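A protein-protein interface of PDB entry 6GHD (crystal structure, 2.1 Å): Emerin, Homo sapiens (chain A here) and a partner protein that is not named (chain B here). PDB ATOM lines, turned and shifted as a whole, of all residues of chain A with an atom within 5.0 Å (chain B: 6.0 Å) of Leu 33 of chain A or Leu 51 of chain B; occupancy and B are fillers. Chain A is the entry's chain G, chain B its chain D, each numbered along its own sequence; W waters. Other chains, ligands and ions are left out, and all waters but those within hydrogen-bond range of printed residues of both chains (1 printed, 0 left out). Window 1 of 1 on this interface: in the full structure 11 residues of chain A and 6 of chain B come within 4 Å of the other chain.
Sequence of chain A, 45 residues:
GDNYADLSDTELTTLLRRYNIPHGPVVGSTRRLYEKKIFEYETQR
OD2 of Asp 54 of chain B lies within hydrogen-bond range of N of Leu 57 of chain B.
The side-chain carboxylate (OD2) of Asp 64 of chain B lies within salt-bridge range of the side-chain amino group (NZ) of Lys 36 of chain A. The side-chain amino group of Lys 37 of chain A is in salt-bridge range of the side-chain carboxylate of Glu 60 of chain B (2.7 Å). The side-chain amino group of Lys 36 of chain A sits close to the side-chain carboxylate of Glu 60 of chain B, at 2.3 Å.
Printed residues of chain B that touch a printed residue of chain A: Val 50, Leu 51, Leu 57, Glu 60 and Asp 64. Hydrophobic or aromatic side chains of chain A that line the printed part of chain B: Leu 33 and Tyr 34. Among the printed residues, 10 pairs touch across the chains.
Water W1 lies within hydrogen-bond range of the backbone carbonyl oxygen of Val 50 of chain B (2.7 Å) and the side-chain hydroxyl of Tyr 34 of chain A (2.8 Å).
Of the printed residues of chain A, Val 50 of chain B touches Thr 30. Of chain A, only Thr 30 (3.8 Å), Leu 33 (3.7 Å) and Tyr 34 (3.6 Å) come within 4 Å of Leu 51 of chain B. Lys 52 of chain B touches none of the printed residues of chain A. Arg 59 of chain B touches none of the printed residues of chain A. Of the printed residues of chain A, Glu 60 of chain B touches Lys 36 and Lys 37. The nearest residue of chain B that does not touch Leu 33 of chain A is Glu 60 of chain B (4.1 Å). The nearest printed residue of chain A that does not touch Leu 51 of chain B is Arg 31 of chain A (7.6 Å). The nearest printed residue of chain A that does not touch Glu 60 of chain B is Leu 33 of chain A (4.1 Å).
Among the printed residues, merely in contact across the chains: Thr 30 of chain A with Val 50 of chain B, Thr 30 of chain A with Leu 51 of chain B, Leu 33 of chain A with Leu 51 of chain B, Leu 33 of chain A with Leu 57 of chain B, Tyr 34 of chain A with Leu 51 of chain B, Tyr 34 of chain A with Leu 57 of chain B and Lys 37 of chain A with Leu 57 of chain B.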
ATOM      1  N   THR A  30     -28.861  25.081  12.854  1.00  0.00           N
ATOM      2  CA  THR A  30     -29.337  24.035  11.965  1.00  0.00           C
ATOM      3  C   THR A  30     -30.546  24.465  11.154  1.00  0.00           C
ATOM      4  O   THR A  30     -30.961  23.737  10.254  1.00  0.00           O
ATOM      5  CB  THR A  30     -29.699  22.771  12.774  1.00  0.00           C
ATOM      6  OG1 THR A  30     -30.775  23.063  13.694  1.00  0.00           O
ATOM      7  CG2 THR A  30     -28.476  22.275  13.558  1.00  0.00           C
ATOM      8  N   ARG A  31     -31.087  25.644  11.443  1.00  0.00           N
ATOM      9  CA  ARG A  31     -32.301  26.129  10.802  1.00  0.00           C
ATOM     10  C   ARG A  31     -32.151  26.181   9.279  1.00  0.00           C
ATOM     11  O   ARG A  31     -32.974  25.624   8.546  1.00  0.00           O
ATOM     12  CB  ARG A  31     -32.619  27.504  11.398  1.00  0.00           C
ATOM     13  CG  ARG A  31     -33.901  28.099  10.959  1.00  0.00           C
ATOM     14  CD  ARG A  31     -34.956  27.210  11.550  1.00  0.00           C
ATOM     15  NE  ARG A  31     -36.129  27.914  12.030  1.00  0.00           N
ATOM     16  CZ  ARG A  31     -37.132  28.310  11.264  1.00  0.00           C
ATOM     17  NH1 ARG A  31     -37.110  28.097   9.955  1.00  0.00           N
ATOM     18  NH2 ARG A  31     -38.160  28.920  11.825  1.00  0.00           N
ATOM     19  N   ARG A  32     -31.082  26.825   8.797  1.00  0.00           N
ATOM     20  CA  ARG A  32     -30.826  26.991   7.364  1.00  0.00           C
ATOM     21  C   ARG A  32     -30.623  25.640   6.676  1.00  0.00           C
ATOM     22  O   ARG A  32     -31.142  25.403   5.578  1.00  0.00           O
ATOM     23  CB  ARG A  32     -29.586  27.891   7.200  1.00  0.00           C
ATOM     24  CG  ARG A  32     -29.185  28.333   5.822  1.00  0.00           C
ATOM     25  CD  ARG A  32     -30.015  29.463   5.224  1.00  0.00           C
ATOM     26  NE  ARG A  32     -29.505  29.774   3.886  1.00  0.00           N
ATOM     27  CZ  ARG A  32     -30.069  30.615   3.023  1.00  0.00           C
ATOM     28  NH1 ARG A  32     -31.185  31.261   3.336  1.00  0.00           N
ATOM     29  NH2 ARG A  32     -29.508  30.817   1.837  1.00  0.00           N
ATOM     30  N   LEU A  33     -29.923  24.716   7.340  1.00  0.00           N
ATOM     31  CA  LEU A  33     -29.687  23.404   6.746  1.00  0.00           C
ATOM     32  C   LEU A  33     -30.995  22.630   6.545  1.00  0.00           C
ATOM     33  O   LEU A  33     -31.201  22.017   5.489  1.00  0.00           O
ATOM     34  CB  LEU A  33     -28.701  22.613   7.620  1.00  0.00           C
ATOM     35  CG  LEU A  33     -28.558  21.091   7.390  1.00  0.00           C
ATOM     36  CD1 LEU A  33     -27.855  20.772   6.060  1.00  0.00           C
ATOM     37  CD2 LEU A  33     -27.815  20.431   8.542  1.00  0.00           C
ATOM     38  N   TYR A  34     -31.904  22.656   7.530  1.00  0.00           N
ATOM     39  CA  TYR A  34     -33.161  21.915   7.398  1.00  0.00           C
ATOM     40  C   TYR A  34     -34.146  22.595   6.456  1.00  0.00           C
ATOM     41  O   TYR A  34     -34.953  21.912   5.816  1.00  0.00           O
ATOM     42  CB  TYR A  34     -33.805  21.708   8.765  1.00  0.00           C
ATOM     43  CG  TYR A  34     -33.022  20.747   9.633  1.00  0.00           C
ATOM     44  CD1 TYR A  34     -32.498  19.580   9.091  1.00  0.00           C
ATOM     45  CD2 TYR A  34     -32.787  21.010  10.977  1.00  0.00           C
ATOM     46  CE1 TYR A  34     -31.762  18.691   9.860  1.00  0.00           C
ATOM     47  CE2 TYR A  34     -32.038  20.115  11.771  1.00  0.00           C
ATOM     48  CZ  TYR A  34     -31.531  18.963  11.193  1.00  0.00           C
ATOM     49  OH  TYR A  34     -30.792  18.059  11.920  1.00  0.00           O
ATOM     50  N   GLU A  35     -34.132  23.930   6.386  1.00  0.00           N
ATOM     51  CA  GLU A  35     -34.933  24.608   5.374  1.00  0.00           C
ATOM     52  C   GLU A  35     -34.573  24.109   3.983  1.00  0.00           C
ATOM     53  O   GLU A  35     -35.443  23.938   3.126  1.00  0.00           O
ATOM     54  CB  GLU A  35     -34.702  26.123   5.443  1.00  0.00           C
ATOM     55  CG  GLU A  35     -35.322  26.856   6.602  1.00  0.00           C
ATOM     56  CD  GLU A  35     -35.108  28.358   6.473  1.00  0.00           C
ATOM     57  OE1 GLU A  35     -35.098  29.061   7.506  1.00  0.00           O
ATOM     58  OE2 GLU A  35     -34.947  28.833   5.323  1.00  0.00           O
ATOM     59  N   LYS A  36     -33.285  23.867   3.753  1.00  0.00           N
ATOM     60  CA  LYS A  36     -32.826  23.414   2.449  1.00  0.00           C
ATOM     61  C   LYS A  36     -33.253  21.975   2.192  1.00  0.00           C
ATOM     62  O   LYS A  36     -33.656  21.632   1.074  1.00  0.00           O
ATOM     63  CB  LYS A  36     -31.312  23.576   2.376  1.00  0.00           C
ATOM     64  CG  LYS A  36     -30.681  23.026   1.136  1.00  0.00           C
ATOM     65  CD  LYS A  36     -29.264  23.536   1.005  1.00  0.00           C
ATOM     66  CE  LYS A  36     -28.420  22.523   0.281  1.00  0.00           C
ATOM     67  NZ  LYS A  36     -28.119  21.414   1.230  1.00  0.00           N
ATOM     68  N   LYS A  37     -33.204  21.128   3.223  1.00  0.00           N
ATOM     69  CA  LYS A  37     -33.649  19.742   3.081  1.00  0.00           C
ATOM     70  C   LYS A  37     -35.119  19.678   2.688  1.00  0.00           C
ATOM     71  O   LYS A  37     -35.509  18.915   1.799  1.00  0.00           O
ATOM     72  CB  LYS A  37     -33.429  18.979   4.395  1.00  0.00           C
ATOM     73  CG  LYS A  37     -31.988  18.892   4.876  1.00  0.00           C
ATOM     74  CD  LYS A  37     -31.355  17.535   4.592  1.00  0.00           C
ATOM     75  CE  LYS A  37     -30.978  17.367   3.144  1.00  0.00           C
ATOM     76  NZ  LYS A  37     -29.923  16.336   3.014  1.00  0.00           N
ATOM     77  N   GLY B  46     -19.755  20.911  18.824  1.00  0.00           N
ATOM     78  CA  GLY B  46     -21.135  21.168  19.195  1.00  0.00           C
ATOM     79  C   GLY B  46     -22.091  20.986  18.040  1.00  0.00           C
ATOM     80  O   GLY B  46     -23.165  20.400  18.189  1.00  0.00           O
ATOM     81  N   GLN B  47     -21.722  21.510  16.869  1.00  0.00           N
ATOM     82  CA  GLN B  47     -22.588  21.357  15.706  1.00  0.00           C
ATOM     83  C   GLN B  47     -22.704  19.890  15.310  1.00  0.00           C
ATOM     84  O   GLN B  47     -23.788  19.395  15.001  1.00  0.00           O
ATOM     85  CB  GLN B  47     -22.026  22.159  14.533  1.00  0.00           C
ATOM     86  CG  GLN B  47     -22.862  22.090  13.274  1.00  0.00           C
ATOM     87  CD  GLN B  47     -24.108  22.949  13.360  1.00  0.00           C
ATOM     88  OE1 GLN B  47     -24.442  23.466  14.419  1.00  0.00           O
ATOM     89  NE2 GLN B  47     -24.794  23.116  12.235  1.00  0.00           N
ATOM     90  N   PHE B  48     -21.583  19.193  15.297  1.00  0.00           N
ATOM     91  CA  PHE B  48     -21.583  17.753  15.076  1.00  0.00           C
ATOM     92  C   PHE B  48     -22.521  17.050  16.061  1.00  0.00           C
ATOM     93  O   PHE B  48     -23.284  16.163  15.673  1.00  0.00           O
ATOM     94  CB  PHE B  48     -20.122  17.290  15.166  1.00  0.00           C
ATOM     95  CG  PHE B  48     -19.912  15.803  15.262  1.00  0.00           C
ATOM     96  CD1 PHE B  48     -19.848  15.018  14.129  1.00  0.00           C
ATOM     97  CD2 PHE B  48     -19.683  15.214  16.496  1.00  0.00           C
ATOM     98  CE1 PHE B  48     -19.605  13.663  14.233  1.00  0.00           C
ATOM     99  CE2 PHE B  48     -19.446  13.852  16.606  1.00  0.00           C
ATOM    100  CZ  PHE B  48     -19.400  13.092  15.465  1.00  0.00           C
ATOM    101  N   LEU B  49     -22.539  17.492  17.333  1.00  0.00           N
ATOM    102  CA  LEU B  49     -23.395  16.835  18.329  1.00  0.00           C
ATOM    103  C   LEU B  49     -24.878  17.179  18.152  1.00  0.00           C
ATOM    104  O   LEU B  49     -25.739  16.317  18.372  1.00  0.00           O
ATOM    105  CB  LEU B  49     -22.924  17.195  19.741  1.00  0.00           C
ATOM    106  CG  LEU B  49     -21.548  16.673  20.187  1.00  0.00           C
ATOM    107  CD1 LEU B  49     -21.227  17.211  21.571  1.00  0.00           C
ATOM    108  CD2 LEU B  49     -21.528  15.138  20.209  1.00  0.00           C
ATOM    109  N   VAL B  50     -25.225  18.430  17.814  1.00  0.00           N
ATOM    110  CA  VAL B  50     -26.651  18.717  17.642  1.00  0.00           C
ATOM    111  C   VAL B  50     -27.201  18.122  16.360  1.00  0.00           C
ATOM    112  O   VAL B  50     -28.420  18.013  16.221  1.00  0.00           O
ATOM    113  CB  VAL B  50     -26.998  20.220  17.673  1.00  0.00           C
ATOM    114  CG1 VAL B  50     -26.680  20.812  19.017  1.00  0.00           C
ATOM    115  CG2 VAL B  50     -26.296  20.967  16.543  1.00  0.00           C
ATOM    116  N   LEU B  51     -26.346  17.813  15.381  1.00  0.00           N
ATOM    117  CA  LEU B  51     -26.740  17.023  14.216  1.00  0.00           C
ATOM    118  C   LEU B  51     -26.744  15.517  14.522  1.00  0.00           C
ATOM    119  O   LEU B  51     -26.878  14.691  13.610  1.00  0.00           O
ATOM    120  CB  LEU B  51     -25.806  17.320  13.044  1.00  0.00           C
ATOM    121  CG  LEU B  51     -25.884  18.751  12.498  1.00  0.00           C
ATOM    122  CD1 LEU B  51     -24.824  18.995  11.435  1.00  0.00           C
ATOM    123  CD2 LEU B  51     -27.283  19.035  11.939  1.00  0.00           C
ATOM    124  N   LYS B  52     -26.613  15.167  15.803  1.00  0.00           N
ATOM    125  CA  LYS B  52     -26.673  13.791  16.275  1.00  0.00           C
ATOM    126  C   LYS B  52     -25.617  12.916  15.606  1.00  0.00           C
ATOM    127  O   LYS B  52     -25.851  11.738  15.330  1.00  0.00           O
ATOM    128  CB  LYS B  52     -28.082  13.221  16.100  1.00  0.00           C
ATOM    129  CG  LYS B  52     -29.087  13.845  17.077  1.00  0.00           C
ATOM    130  CD  LYS B  52     -30.272  12.926  17.281  1.00  0.00           C
ATOM    131  CE  LYS B  52     -31.375  13.612  18.053  1.00  0.00           C
ATOM    132  NZ  LYS B  52     -32.576  12.759  18.232  1.00  0.00           N
ATOM    133  N   LYS B  53     -24.427  13.494  15.388  1.00  0.00           N
ATOM    134  CA  LYS B  53     -23.262  12.779  14.872  1.00  0.00           C
ATOM    135  C   LYS B  53     -23.517  12.197  13.485  1.00  0.00           C
ATOM    136  O   LYS B  53     -22.785  11.321  13.039  1.00  0.00           O
ATOM    137  CB  LYS B  53     -22.825  11.661  15.844  1.00  0.00           C
ATOM    138  CG  LYS B  53     -22.675  12.092  17.337  1.00  0.00           C
ATOM    139  CD  LYS B  53     -22.261  10.894  18.222  1.00  0.00           C
ATOM    140  CE  LYS B  53     -22.111  11.286  19.698  1.00  0.00           C
ATOM    141  NZ  LYS B  53     -22.514  10.155  20.609  1.00  0.00           N
ATOM    142  N   ASP B  54     -24.533  12.689  12.777  1.00  0.00           N
ATOM    143  CA  ASP B  54     -24.871  12.146  11.467  1.00  0.00           C
ATOM    144  C   ASP B  54     -23.901  12.667  10.409  1.00  0.00           C
ATOM    145  O   ASP B  54     -23.691  13.879  10.294  1.00  0.00           O
ATOM    146  CB  ASP B  54     -26.308  12.498  11.086  1.00  0.00           C
ATOM    147  CG  ASP B  54     -26.736  11.846   9.784  1.00  0.00           C
ATOM    148  OD1 ASP B  54     -27.082  10.637   9.821  1.00  0.00           O
ATOM    149  OD2 ASP B  54     -26.722  12.530   8.735  1.00  0.00           O
ATOM    150  N   LEU B  57     -25.592  14.857   7.311  1.00  0.00           N
ATOM    151  CA  LEU B  57     -26.001  16.194   7.749  1.00  0.00           C
ATOM    152  C   LEU B  57     -24.798  17.066   8.075  1.00  0.00           C
ATOM    153  O   LEU B  57     -24.763  18.247   7.714  1.00  0.00           O
ATOM    154  CB  LEU B  57     -26.948  16.112   8.946  1.00  0.00           C
ATOM    155  CG  LEU B  57     -28.332  15.593   8.562  1.00  0.00           C
ATOM    156  CD1 LEU B  57     -29.215  15.473   9.778  1.00  0.00           C
ATOM    157  CD2 LEU B  57     -28.966  16.517   7.531  1.00  0.00           C
ATOM    158  N   PHE B  58     -23.795  16.502   8.744  1.00  0.00           N
ATOM    159  CA  PHE B  58     -22.631  17.295   9.124  1.00  0.00           C
ATOM    160  C   PHE B  58     -21.831  17.740   7.911  1.00  0.00           C
ATOM    161  O   PHE B  58     -21.355  18.885   7.850  1.00  0.00           O
ATOM    162  CB  PHE B  58     -21.737  16.501  10.076  1.00  0.00           C
ATOM    163  CG  PHE B  58     -20.485  17.240  10.488  1.00  0.00           C
ATOM    164  CD1 PHE B  58     -20.524  18.198  11.494  1.00  0.00           C
ATOM    165  CD2 PHE B  58     -19.278  16.983   9.857  1.00  0.00           C
ATOM    166  CE1 PHE B  58     -19.386  18.867  11.884  1.00  0.00           C
ATOM    167  CE2 PHE B  58     -18.125  17.659  10.235  1.00  0.00           C
ATOM    168  CZ  PHE B  58     -18.182  18.605  11.247  1.00  0.00           C
ATOM    169  N   ARG B  59     -21.575  16.819   6.983  1.00  0.00           N
ATOM    170  CA  ARG B  59     -20.749  17.182   5.835  1.00  0.00           C
ATOM    171  C   ARG B  59     -21.479  18.169   4.931  1.00  0.00           C
ATOM    172  O   ARG B  59     -20.855  19.046   4.324  1.00  0.00           O
ATOM    173  CB  ARG B  59     -20.335  15.933   5.067  1.00  0.00           C
ATOM    174  CG  ARG B  59     -19.500  15.023   5.929  1.00  0.00           C
ATOM    175  CD  ARG B  59     -19.091  13.768   5.207  1.00  0.00           C
ATOM    176  NE  ARG B  59     -18.236  14.061   4.069  1.00  0.00           N
ATOM    177  CZ  ARG B  59     -17.838  13.141   3.199  1.00  0.00           C
ATOM    178  NH1 ARG B  59     -18.229  11.884   3.341  1.00  0.00           N
ATOM    179  NH2 ARG B  59     -17.051  13.476   2.191  1.00  0.00           N
ATOM    180  N   GLU B  60     -22.800  18.016   4.798  1.00  0.00           N
ATOM    181  CA  GLU B  60     -23.564  18.981   4.013  1.00  0.00           C
ATOM    182  C   GLU B  60     -23.564  20.356   4.683  1.00  0.00           C
ATOM    183  O   GLU B  60     -23.517  21.385   4.001  1.00  0.00           O
ATOM    184  CB  GLU B  60     -24.978  18.449   3.788  1.00  0.00           C
ATOM    185  CG  GLU B  60     -25.816  19.268   2.789  1.00  0.00           C
ATOM    186  CD  GLU B  60     -27.230  18.716   2.603  1.00  0.00           C
ATOM    187  OE1 GLU B  60     -27.604  17.763   3.324  1.00  0.00           O
ATOM    188  OE2 GLU B  60     -27.966  19.218   1.721  1.00  0.00           O
ATOM    189  N   TRP B  61     -23.613  20.397   6.021  1.00  0.00           N
ATOM    190  CA  TRP B  61     -23.539  21.673   6.730  1.00  0.00           C
ATOM    191  C   TRP B  61     -22.172  22.331   6.553  1.00  0.00           C
ATOM    192  O   TRP B  61     -22.077  23.548   6.315  1.00  0.00           O
ATOM    193  CB  TRP B  61     -23.846  21.480   8.219  1.00  0.00           C
ATOM    194  CG  TRP B  61     -23.440  22.667   8.982  1.00  0.00           C
ATOM    195  CD1 TRP B  61     -24.131  23.839   9.101  1.00  0.00           C
ATOM    196  CD2 TRP B  61     -22.218  22.841   9.701  1.00  0.00           C
ATOM    197  NE1 TRP B  61     -23.412  24.734   9.863  1.00  0.00           N
ATOM    198  CE2 TRP B  61     -22.232  24.146  10.241  1.00  0.00           C
ATOM    199  CE3 TRP B  61     -21.117  22.012   9.962  1.00  0.00           C
ATOM    200  CZ2 TRP B  61     -21.193  24.639  11.038  1.00  0.00           C
ATOM    201  CZ3 TRP B  61     -20.080  22.506  10.742  1.00  0.00           C
ATOM    202  CH2 TRP B  61     -20.127  23.809  11.273  1.00  0.00           C
ATOM    203  N   ASP B  64     -21.886  23.742   3.007  1.00  0.00           N
ATOM    204  CA  ASP B  64     -22.703  24.906   2.712  1.00  0.00           C
ATOM    205  C   ASP B  64     -22.310  26.115   3.557  1.00  0.00           C
ATOM    206  O   ASP B  64     -22.466  27.254   3.106  1.00  0.00           O
ATOM    207  CB  ASP B  64     -24.184  24.577   2.911  1.00  0.00           C
ATOM    208  CG  ASP B  64     -24.721  23.653   1.833  1.00  0.00           C
ATOM    209  OD1 ASP B  64     -24.299  23.808   0.669  1.00  0.00           O
ATOM    210  OD2 ASP B  64     -25.595  22.810   2.122  1.00  0.00           O
HETATM  211  O   HOH W   1     -29.998  19.181  14.407  1.00  0.00           O
